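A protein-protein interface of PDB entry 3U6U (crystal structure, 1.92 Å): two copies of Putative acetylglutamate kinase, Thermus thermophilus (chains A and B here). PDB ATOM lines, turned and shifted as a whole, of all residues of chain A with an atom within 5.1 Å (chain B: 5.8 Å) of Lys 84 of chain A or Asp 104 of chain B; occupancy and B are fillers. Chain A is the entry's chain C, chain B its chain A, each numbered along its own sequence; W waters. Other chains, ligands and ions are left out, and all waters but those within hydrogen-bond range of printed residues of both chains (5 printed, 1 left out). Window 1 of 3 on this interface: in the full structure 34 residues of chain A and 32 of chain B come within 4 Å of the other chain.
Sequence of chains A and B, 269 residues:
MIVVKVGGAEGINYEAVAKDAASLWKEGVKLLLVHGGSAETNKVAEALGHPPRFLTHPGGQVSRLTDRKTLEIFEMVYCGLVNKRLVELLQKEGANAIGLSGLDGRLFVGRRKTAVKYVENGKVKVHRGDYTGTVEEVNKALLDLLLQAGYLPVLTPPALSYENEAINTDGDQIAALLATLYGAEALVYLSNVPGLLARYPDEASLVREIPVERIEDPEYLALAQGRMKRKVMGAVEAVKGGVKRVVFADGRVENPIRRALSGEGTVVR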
ATOM      1  N   CYS A  79       4.217 -31.888 -13.564  1.00  0.00           N
ATOM      2  CA  CYS A  79       4.448 -31.290 -14.875  1.00  0.00           C
ATOM      3  C   CYS A  79       4.388 -29.772 -14.935  1.00  0.00           C
ATOM      4  O   CYS A  79       4.986 -29.166 -15.824  1.00  0.00           O
ATOM      5  CB  CYS A  79       3.455 -31.868 -15.882  1.00  0.00           C
ATOM      6  SG  CYS A  79       3.344 -33.660 -15.808  1.00  0.00           S
ATOM      7  N   GLY A  80       3.655 -29.160 -14.009  1.00  0.00           N
ATOM      8  CA  GLY A  80       3.560 -27.714 -14.011  1.00  0.00           C
ATOM      9  C   GLY A  80       4.471 -27.054 -12.989  1.00  0.00           C
ATOM     10  O   GLY A  80       5.483 -26.457 -13.339  1.00  0.00           O
ATOM     11  N   LEU A  81       4.119 -27.188 -11.716  1.00  0.00           N
ATOM     12  CA  LEU A  81       4.878 -26.576 -10.635  1.00  0.00           C
ATOM     13  C   LEU A  81       6.358 -26.948 -10.558  1.00  0.00           C
ATOM     14  O   LEU A  81       7.229 -26.100 -10.746  1.00  0.00           O
ATOM     15  CB  LEU A  81       4.221 -26.900  -9.289  1.00  0.00           C
ATOM     16  CG  LEU A  81       4.766 -26.176  -8.053  1.00  0.00           C
ATOM     17  CD1 LEU A  81       4.370 -24.703  -8.100  1.00  0.00           C
ATOM     18  CD2 LEU A  81       4.206 -26.824  -6.795  1.00  0.00           C
ATOM     19  N   VAL A  82       6.638 -28.212 -10.265  1.00  0.00           N
ATOM     20  CA  VAL A  82       8.012 -28.655 -10.107  1.00  0.00           C
ATOM     21  C   VAL A  82       8.847 -28.612 -11.385  1.00  0.00           C
ATOM     22  O   VAL A  82       9.957 -28.079 -11.385  1.00  0.00           O
ATOM     23  CB  VAL A  82       8.063 -30.076  -9.504  1.00  0.00           C
ATOM     24  CG1 VAL A  82       9.508 -30.481  -9.236  1.00  0.00           C
ATOM     25  CG2 VAL A  82       7.267 -30.110  -8.195  1.00  0.00           C
ATOM     26  N   ASN A  83       8.314 -29.153 -12.475  1.00  0.00           N
ATOM     27  CA  ASN A  83       9.055 -29.169 -13.733  1.00  0.00           C
ATOM     28  C   ASN A  83       9.472 -27.766 -14.175  1.00  0.00           C
ATOM     29  O   ASN A  83      10.638 -27.535 -14.490  1.00  0.00           O
ATOM     30  CB  ASN A  83       8.223 -29.839 -14.840  1.00  0.00           C
ATOM     31  CG  ASN A  83       9.043 -30.132 -16.098  1.00  0.00           C
ATOM     32  OD1 ASN A  83       8.869 -29.483 -17.131  1.00  0.00           O
ATOM     33  ND2 ASN A  83       9.939 -31.116 -16.011  1.00  0.00           N
ATOM     34  N   LYS A  84       8.534 -26.822 -14.182  1.00  0.00           N
ATOM     35  CA  LYS A  84       8.865 -25.472 -14.625  1.00  0.00           C
ATOM     36  C   LYS A  84       9.679 -24.684 -13.604  1.00  0.00           C
ATOM     37  O   LYS A  84      10.401 -23.761 -13.967  1.00  0.00           O
ATOM     38  CB  LYS A  84       7.591 -24.709 -15.026  1.00  0.00           C
ATOM     39  CG  LYS A  84       6.726 -25.444 -16.077  1.00  0.00           C
ATOM     40  CD  LYS A  84       7.553 -26.057 -17.228  1.00  0.00           C
ATOM     41  CE  LYS A  84       6.671 -26.926 -18.143  1.00  0.00           C
ATOM     42  NZ  LYS A  84       7.426 -27.669 -19.212  1.00  0.00           N
ATOM     43  N   ARG A  85       9.568 -25.046 -12.328  1.00  0.00           N
ATOM     44  CA  ARG A  85      10.356 -24.386 -11.291  1.00  0.00           C
ATOM     45  C   ARG A  85      11.825 -24.707 -11.572  1.00  0.00           C
ATOM     46  O   ARG A  85      12.683 -23.820 -11.605  1.00  0.00           O
ATOM     47  CB  ARG A  85       9.997 -24.926  -9.901  1.00  0.00           C
ATOM     48  CG  ARG A  85      10.971 -24.485  -8.803  1.00  0.00           C
ATOM     49  CD  ARG A  85      10.787 -25.299  -7.534  1.00  0.00           C
ATOM     50  NE  ARG A  85       9.446 -25.126  -6.983  1.00  0.00           N
ATOM     51  CZ  ARG A  85       8.794 -26.060  -6.301  1.00  0.00           C
ATOM     52  NH1 ARG A  85       9.354 -27.242  -6.083  1.00  0.00           N
ATOM     53  NH2 ARG A  85       7.578 -25.808  -5.835  1.00  0.00           N
ATOM     54  N   LEU A  86      12.090 -25.991 -11.782  1.00  0.00           N
ATOM     55  CA  LEU A  86      13.435 -26.487 -12.045  1.00  0.00           C
ATOM     56  C   LEU A  86      14.000 -25.972 -13.378  1.00  0.00           C
ATOM     57  O   LEU A  86      15.163 -25.567 -13.455  1.00  0.00           O
ATOM     58  CB  LEU A  86      13.415 -28.023 -12.003  1.00  0.00           C
ATOM     59  CG  LEU A  86      14.719 -28.814 -11.896  1.00  0.00           C
ATOM     60  CD1 LEU A  86      15.605 -28.241 -10.789  1.00  0.00           C
ATOM     61  CD2 LEU A  86      14.384 -30.277 -11.607  1.00  0.00           C
ATOM     62  N   VAL A  87      13.188 -25.977 -14.428  1.00  0.00           N
ATOM     63  CA  VAL A  87      13.655 -25.470 -15.715  1.00  0.00           C
ATOM     64  C   VAL A  87      14.099 -24.003 -15.565  1.00  0.00           C
ATOM     65  O   VAL A  87      15.172 -23.617 -16.038  1.00  0.00           O
ATOM     66  CB  VAL A  87      12.544 -25.588 -16.789  1.00  0.00           C
ATOM     67  CG1 VAL A  87      12.948 -24.845 -18.063  1.00  0.00           C
ATOM     68  CG2 VAL A  87      12.296 -27.063 -17.102  1.00  0.00           C
ATOM     69  N   GLU A  88      13.281 -23.193 -14.893  1.00  0.00           N
ATOM     70  CA  GLU A  88      13.615 -21.782 -14.686  1.00  0.00           C
ATOM     71  C   GLU A  88      14.900 -21.610 -13.875  1.00  0.00           C
ATOM     72  O   GLU A  88      15.752 -20.795 -14.226  1.00  0.00           O
ATOM     73  CB  GLU A  88      12.467 -21.049 -13.980  1.00  0.00           C
ATOM     74  CG  GLU A  88      12.841 -19.640 -13.509  1.00  0.00           C
ATOM     75  CD  GLU A  88      11.703 -18.937 -12.787  1.00  0.00           C
ATOM     76  OE1 GLU A  88      10.898 -19.630 -12.129  1.00  0.00           O
ATOM     77  OE2 GLU A  88      11.622 -17.693 -12.866  1.00  0.00           O
ATOM     78  N   LEU A  89      15.033 -22.374 -12.792  1.00  0.00           N
ATOM     79  CA  LEU A  89      16.224 -22.304 -11.946  1.00  0.00           C
ATOM     80  C   LEU A  89      17.471 -22.634 -12.763  1.00  0.00           C
ATOM     81  O   LEU A  89      18.512 -21.985 -12.623  1.00  0.00           O
ATOM     82  CB  LEU A  89      16.104 -23.275 -10.769  1.00  0.00           C
ATOM     83  CG  LEU A  89      15.097 -22.885  -9.676  1.00  0.00           C
ATOM     84  CD1 LEU A  89      15.014 -23.993  -8.629  1.00  0.00           C
ATOM     85  CD2 LEU A  89      15.523 -21.568  -9.028  1.00  0.00           C
ATOM     86  N   GLN A  91      17.787 -22.370 -16.111  1.00  0.00           N
ATOM     87  CA  GLN A  91      18.031 -21.301 -17.080  1.00  0.00           C
ATOM     88  C   GLN A  91      18.715 -20.125 -16.375  1.00  0.00           C
ATOM     89  O   GLN A  91      19.591 -19.476 -16.946  1.00  0.00           O
ATOM     90  CB  GLN A  91      16.722 -20.823 -17.722  1.00  0.00           C
ATOM     91  CG  GLN A  91      16.047 -21.839 -18.654  1.00  0.00           C
ATOM     92  CD  GLN A  91      16.816 -22.075 -19.957  1.00  0.00           C
ATOM     93  OE1 GLN A  91      17.778 -21.365 -20.274  1.00  0.00           O
ATOM     94  NE2 GLN A  91      16.378 -23.068 -20.724  1.00  0.00           N
ATOM     95  N   ALA A  97      17.901 -25.790 -20.046  1.00  0.00           N
ATOM     96  CA  ALA A  97      17.001 -26.870 -19.694  1.00  0.00           C
ATOM     97  C   ALA A  97      15.718 -26.918 -20.525  1.00  0.00           C
ATOM     98  O   ALA A  97      15.159 -25.888 -20.909  1.00  0.00           O
ATOM     99  CB  ALA A  97      16.647 -26.766 -18.201  1.00  0.00           C
ATOM    100  N   ILE A  98      15.261 -28.135 -20.799  1.00  0.00           N
ATOM    101  CA  ILE A  98      14.021 -28.335 -21.530  1.00  0.00           C
ATOM    102  C   ILE A  98      13.236 -29.362 -20.715  1.00  0.00           C
ATOM    103  O   ILE A  98      13.693 -30.481 -20.497  1.00  0.00           O
ATOM    104  CB  ILE A  98      14.274 -28.827 -22.987  1.00  0.00           C
ATOM    105  CG1 ILE A  98      12.952 -28.890 -23.749  1.00  0.00           C
ATOM    106  CG2 ILE A  98      14.947 -30.198 -22.990  1.00  0.00           C
ATOM    107  CD1 ILE A  98      13.135 -29.048 -25.259  1.00  0.00           C
ATOM    108  N   GLY A  99      12.064 -28.959 -20.231  1.00  0.00           N
ATOM    109  CA  GLY A  99      11.259 -29.855 -19.413  1.00  0.00           C
ATOM    110  C   GLY A  99      10.259 -30.669 -20.204  1.00  0.00           C
ATOM    111  O   GLY A  99       9.567 -30.124 -21.060  1.00  0.00           O
ATOM    112  N   GLU B  75       1.360 -21.742 -13.796  1.00  0.00           N
ATOM    113  CA  GLU B  75       2.143 -22.841 -14.356  1.00  0.00           C
ATOM    114  C   GLU B  75       1.456 -24.183 -14.119  1.00  0.00           C
ATOM    115  O   GLU B  75       1.374 -25.010 -15.025  1.00  0.00           O
ATOM    116  CB  GLU B  75       3.558 -22.842 -13.768  1.00  0.00           C
ATOM    117  CG  GLU B  75       4.372 -21.621 -14.181  1.00  0.00           C
ATOM    118  CD  GLU B  75       5.766 -21.601 -13.584  1.00  0.00           C
ATOM    119  OE1 GLU B  75       5.935 -22.074 -12.445  1.00  0.00           O
ATOM    120  OE2 GLU B  75       6.693 -21.090 -14.249  1.00  0.00           O
ATOM    121  N   CYS B  79       0.774 -25.102 -17.852  1.00  0.00           N
ATOM    122  CA  CYS B  79       1.835 -26.053 -18.169  1.00  0.00           C
ATOM    123  C   CYS B  79       1.588 -27.492 -17.744  1.00  0.00           C
ATOM    124  O   CYS B  79       2.112 -28.423 -18.362  1.00  0.00           O
ATOM    125  CB  CYS B  79       3.149 -25.564 -17.556  1.00  0.00           C
ATOM    126  SG  CYS B  79       3.521 -23.840 -17.955  1.00  0.00           S
ATOM    127  N   LYS B  84      -0.716 -30.965 -20.668  1.00  0.00           N
ATOM    128  CA  LYS B  84      -0.678 -32.423 -20.677  1.00  0.00           C
ATOM    129  C   LYS B  84      -2.008 -33.053 -21.077  1.00  0.00           C
ATOM    130  O   LYS B  84      -2.035 -34.155 -21.627  1.00  0.00           O
ATOM    131  CB  LYS B  84      -0.209 -32.949 -19.317  1.00  0.00           C
ATOM    132  CG  LYS B  84       1.131 -32.349 -18.878  1.00  0.00           C
ATOM    133  CD  LYS B  84       2.129 -32.264 -20.033  1.00  0.00           C
ATOM    134  CE  LYS B  84       3.391 -31.486 -19.630  1.00  0.00           C
ATOM    135  NZ  LYS B  84       4.284 -31.215 -20.798  1.00  0.00           N
ATOM    136  N   GLY B  99       4.558 -31.266 -25.736  1.00  0.00           N
ATOM    137  CA  GLY B  99       4.177 -30.024 -25.086  1.00  0.00           C
ATOM    138  C   GLY B  99       5.349 -29.266 -24.493  1.00  0.00           C
ATOM    139  O   GLY B  99       6.202 -29.854 -23.828  1.00  0.00           O
ATOM    140  N   LEU B 100       5.388 -27.958 -24.733  1.00  0.00           N
ATOM    141  CA  LEU B 100       6.462 -27.116 -24.222  1.00  0.00           C
ATOM    142  C   LEU B 100       5.954 -25.757 -23.768  1.00  0.00           C
ATOM    143  O   LEU B 100       5.017 -25.211 -24.353  1.00  0.00           O
ATOM    144  CB  LEU B 100       7.508 -26.861 -25.307  1.00  0.00           C
ATOM    145  CG  LEU B 100       8.272 -28.038 -25.908  1.00  0.00           C
ATOM    146  CD1 LEU B 100       9.038 -27.562 -27.138  1.00  0.00           C
ATOM    147  CD2 LEU B 100       9.217 -28.613 -24.864  1.00  0.00           C
ATOM    148  N   SER B 101       6.590 -25.210 -22.735  1.00  0.00           N
ATOM    149  CA  SER B 101       6.247 -23.877 -22.260  1.00  0.00           C
ATOM    150  C   SER B 101       7.362 -22.988 -22.811  1.00  0.00           C
ATOM    151  O   SER B 101       8.361 -23.493 -23.339  1.00  0.00           O
ATOM    152  CB  SER B 101       6.253 -23.812 -20.731  1.00  0.00           C
ATOM    153  OG  SER B 101       7.575 -23.673 -20.237  1.00  0.00           O
ATOM    154  N   GLY B 102       7.198 -21.674 -22.696  1.00  0.00           N
ATOM    155  CA  GLY B 102       8.214 -20.766 -23.196  1.00  0.00           C
ATOM    156  C   GLY B 102       9.548 -20.872 -22.471  1.00  0.00           C
ATOM    157  O   GLY B 102      10.577 -20.443 -22.999  1.00  0.00           O
ATOM    158  N   LEU B 103       9.536 -21.436 -21.265  1.00  0.00           N
ATOM    159  CA  LEU B 103      10.753 -21.591 -20.467  1.00  0.00           C
ATOM    160  C   LEU B 103      11.661 -22.688 -21.013  1.00  0.00           C
ATOM    161  O   LEU B 103      12.889 -22.612 -20.921  1.00  0.00           O
ATOM    162  CB  LEU B 103      10.397 -21.968 -19.030  1.00  0.00           C
ATOM    163  CG  LEU B 103       9.359 -21.124 -18.296  1.00  0.00           C
ATOM    164  CD1 LEU B 103       9.144 -21.715 -16.916  1.00  0.00           C
ATOM    165  CD2 LEU B 103       9.832 -19.673 -18.208  1.00  0.00           C
ATOM    166  N   ASP B 104      11.033 -23.715 -21.568  1.00  0.00           N
ATOM    167  CA  ASP B 104      11.746 -24.875 -22.081  1.00  0.00           C
ATOM    168  C   ASP B 104      12.601 -24.585 -23.307  1.00  0.00           C
ATOM    169  O   ASP B 104      12.101 -24.135 -24.336  1.00  0.00           O
ATOM    170  CB  ASP B 104      10.717 -25.981 -22.335  1.00  0.00           C
ATOM    171  CG  ASP B 104       9.941 -26.319 -21.072  1.00  0.00           C
ATOM    172  OD1 ASP B 104      10.587 -26.771 -20.103  1.00  0.00           O
ATOM    173  OD2 ASP B 104       8.706 -26.113 -21.032  1.00  0.00           O
ATOM    174  N   GLY B 105      13.903 -24.836 -23.172  1.00  0.00           N
ATOM    175  CA  GLY B 105      14.832 -24.572 -24.259  1.00  0.00           C
ATOM    176  C   GLY B 105      14.783 -23.105 -24.648  1.00  0.00           C
ATOM    177  O   GLY B 105      15.164 -22.735 -25.756  1.00  0.00           O
ATOM    178  N   ARG B 106      14.322 -22.265 -23.725  1.00  0.00           N
ATOM    179  CA  ARG B 106      14.193 -20.827 -23.979  1.00  0.00           C
ATOM    180  C   ARG B 106      13.349 -20.597 -25.228  1.00  0.00           C
ATOM    181  O   ARG B 106      13.653 -19.745 -26.062  1.00  0.00           O
ATOM    182  CB  ARG B 106      15.573 -20.179 -24.143  1.00  0.00           C
ATOM    183  CG  ARG B 106      16.454 -20.336 -22.917  1.00  0.00           C
ATOM    184  CD  ARG B 106      17.531 -19.261 -22.863  1.00  0.00           C
ATOM    185  NE  ARG B 106      18.658 -19.512 -23.757  1.00  0.00           N
ATOM    186  CZ  ARG B 106      19.657 -20.352 -23.490  1.00  0.00           C
ATOM    187  NH1 ARG B 106      19.671 -21.033 -22.352  1.00  0.00           N
ATOM    188  NH2 ARG B 106      20.662 -20.492 -24.352  1.00  0.00           N
ATOM    189  N   LEU B 107      12.279 -21.374 -25.343  1.00  0.00           N
ATOM    190  CA  LEU B 107      11.377 -21.279 -26.484  1.00  0.00           C
ATOM    191  C   LEU B 107      10.817 -19.871 -26.718  1.00  0.00           C
ATOM    192  O   LEU B 107      10.789 -19.398 -27.854  1.00  0.00           O
ATOM    193  CB  LEU B 107      10.224 -22.267 -26.308  1.00  0.00           C
ATOM    194  CG  LEU B 107       9.111 -22.215 -27.358  1.00  0.00           C
ATOM    195  CD1 LEU B 107       9.676 -22.460 -28.744  1.00  0.00           C
ATOM    196  CD2 LEU B 107       8.057 -23.254 -27.012  1.00  0.00           C
ATOM    197  N   PHE B 108      10.359 -19.214 -25.653  1.00  0.00           N
ATOM    198  CA  PHE B 108       9.807 -17.857 -25.767  1.00  0.00           C
ATOM    199  C   PHE B 108      10.538 -16.924 -24.803  1.00  0.00           C
ATOM    200  O   PHE B 108      10.531 -17.140 -23.591  1.00  0.00           O
ATOM    201  CB  PHE B 108       8.303 -17.833 -25.446  1.00  0.00           C
ATOM    202  CG  PHE B 108       7.461 -18.700 -26.351  1.00  0.00           C
ATOM    203  CD1 PHE B 108       7.645 -18.686 -27.731  1.00  0.00           C
ATOM    204  CD2 PHE B 108       6.473 -19.521 -25.817  1.00  0.00           C
ATOM    205  CE1 PHE B 108       6.853 -19.485 -28.568  1.00  0.00           C
ATOM    206  CE2 PHE B 108       5.678 -20.321 -26.642  1.00  0.00           C
ATOM    207  CZ  PHE B 108       5.867 -20.303 -28.019  1.00  0.00           C
ATOM    208  N   ASN B 139      12.566 -19.554 -30.069  1.00  0.00           N
ATOM    209  CA  ASN B 139      13.616 -20.502 -30.422  1.00  0.00           C
ATOM    210  C   ASN B 139      13.069 -21.303 -31.602  1.00  0.00           C
ATOM    211  O   ASN B 139      12.637 -22.456 -31.456  1.00  0.00           O
ATOM    212  CB  ASN B 139      13.927 -21.453 -29.266  1.00  0.00           C
ATOM    213  CG  ASN B 139      15.146 -22.315 -29.547  1.00  0.00           C
ATOM    214  OD1 ASN B 139      15.531 -22.499 -30.703  1.00  0.00           O
ATOM    215  ND2 ASN B 139      15.753 -22.852 -28.498  1.00  0.00           N
ATOM    216  N   LEU B 142      14.612 -24.777 -32.357  1.00  0.00           N
ATOM    217  CA  LEU B 142      14.097 -25.899 -31.574  1.00  0.00           C
ATOM    218  C   LEU B 142      12.794 -26.431 -32.175  1.00  0.00           C
ATOM    219  O   LEU B 142      12.608 -27.642 -32.291  1.00  0.00           O
ATOM    220  CB  LEU B 142      13.855 -25.478 -30.124  1.00  0.00           C
ATOM    221  CG  LEU B 142      13.124 -26.499 -29.240  1.00  0.00           C
ATOM    222  CD1 LEU B 142      13.909 -27.815 -29.185  1.00  0.00           C
ATOM    223  CD2 LEU B 142      12.964 -25.919 -27.841  1.00  0.00           C
HETATM  224  O   HOH W   1       6.951 -23.459 -10.346  1.00  0.00           O
HETATM  225  O   HOH W   2       6.839 -29.730 -21.227  1.00  0.00           O
HETATM  226  O   HOH W   3      20.120 -20.066 -19.523  1.00  0.00           O
HETATM  227  O   HOH W   4       6.147 -30.581 -18.048  1.00  0.00           O
HETATM  228  O   HOH W   5       4.347 -27.877 -20.061  1.00  0.00           O
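Among the printed residues, pairs that only touch across the chains: Cys 79 of chain A with Cys 79 of chain B (3.9 Å), Cys 79 of chain A with Lys 84 of chain B (3.8 Å), Gly 80 of chain A with Glu 75 of chain B (3.6 Å), Lys 84 of chain A with Glu 75 of chain B (3.8 Å), Lys 84 of chain A with Cys 79 of chain B (3.8 Å), Lys 84 of chain A with Ser 101 of chain B (3.8 Å), Lys 84 of chain A with Leu 103 of chain B (3.8 Å), Val 87 of chain A with Leu 103 of chain B (3.6 Å), Val 87 of chain A with Asp 104 of chain B (3.5 Å), Gln 91 of chain A with Leu 103 of chain B (3.5 Å), Gln 91 of chain A with Gly 105 of chain B (3.9 Å), Ala 97 of chain A with Leu 103 of chain B (3.99 Å), Ala 97 of chain A with Asp 104 of chain B (3.7 Å), Ile 98 of chain A with Leu 100 of chain B (3.9 Å), Ile 98 of chain A with Asp 104 of chain B (3.8 Å) and Ile 98 of chain A with Gly 105 of chain B (3.9 Å).
The guanidinium group (NH1) of Arg 106 of chain B is in hydrogen-bond range of the side-chain amide oxygen (OE1) of Gln 91 of chain A, at 2.8 Å.
O of Ala 97 of chain A sits at hydrogen-bond distance from N of Gly 105 of chain B.
NZ of Lys 84 of chain A lies within salt-bridge range of OD2 of Asp 104 of chain B, at 2.7 Å.
OD1 of Asp 104 of chain B sits at hydrogen-bond distance from N of Gly 99 of chain A (2.6 Å).
Lys 84 of chain A touches five residues of chain B.
Of the printed residues of chain B, Gly 99 of chain A touches Asp 104.
Of the printed residues of chain A, Cys 79 of chain B touches Cys 79 (3.9 Å) and Lys 84 (3.8 Å).
Printed residues of chain A within 4 Å of Lys 84 of chain B: Cys 79.
Asp 104 of chain B touches just these residues of chain A: Lys 84 (2.7 Å), Val 87 (3.5 Å), Ala 97 (3.7 Å), Ile 98 (3.8 Å) and Gly 99 (2.6 Å).
Leu 142 of chain B touches none of the printed residues of chain A.
The nearest residue of chain B that does not touch Lys 84 of chain A is Lys 84 of chain B (5.0 Å).
The nearest residue of chain A that does not touch Asp 104 of chain B is Asn 83 of chain A (4.4 Å).
NE2 of Gln 91 of chain A lies within hydrogen-bond range of O of Ala 97 of chain A (3.1 Å).
OG of Ser 101 of chain B lies close to N of Leu 103 of chain B (3.1 Å).
OG of Ser 101 of chain B lies within hydrogen-bond range of OD2 of Asp 104 of chain B.
The side-chain amide oxygen of Asn 83 of chain A is in hydrogen-bond range of the side-chain amino group of Lys 84 of chain A.
ND2 of Asn 139 of chain B lies within hydrogen-bond range of O of Gly 105 of chain B (2.8 Å).
Cys 79 of chain B touches its own counterpart, Cys 79 of chain A.
Cys 79 of chain A touches Lys 84 of chain B, and with the chains exchanged Lys 84 of chain A touches Cys 79 of chain B.
Positions printed for both chains: 79, 84 and 99.
Of the 20 pairs that touch across the chains among the printed residues, 3 have their exchanged pair printed and touching as well.
Water W2 lies within hydrogen-bond range of the backbone carbonyl oxygen of Gly 99 of chain B, the backbone carbonyl oxygen of Gly 99 of chain A, the side-chain amino group of Lys 84 of chain A and the side-chain amino group of Lys 84 of chain B.
Water W1 lies within hydrogen-bond range of the backbone carbonyl oxygen of Leu 81 of chain A (2.7 Å) and the side-chain carboxylate of Glu 75 of chain B (2.7 Å).
Water W3 bridges O of Gln 91 of chain A (2.7 Å) and NH1 of Arg 106 of chain B (3.0 Å).
Water W5 lies within hydrogen-bond range of the backbone carbonyl oxygen of Cys 79 of chain B (2.9 Å), the side-chain amino group of Lys 84 of chain A (3.2 Å) and the side-chain amino group of Lys 84 of chain B (3.4 Å).
Water W4 lies within hydrogen-bond range of the backbone carbonyl oxygen of Cys 79 of chain A (2.9 Å), the side-chain amide oxygen of Asn 83 of chain A (3.1 Å), the side-chain amino group of Lys 84 of chain B (3.4 Å) and the side-chain amino group of Lys 84 of chain A (3.4 Å).
Hydrophobic or aromatic side chains of chain A within 4 Å of the printed part of chain B: Val 87 and Ile 98.
Among the printed residues, 20 pairs touch across the chains.
Among the printed residues, Asp or Glu carboxylates within 4 Å of a Lys or Arg side-chain nitrogen of the other chain: Lys 84 of chain A with Asp 104 of chain B (2.7 Å).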
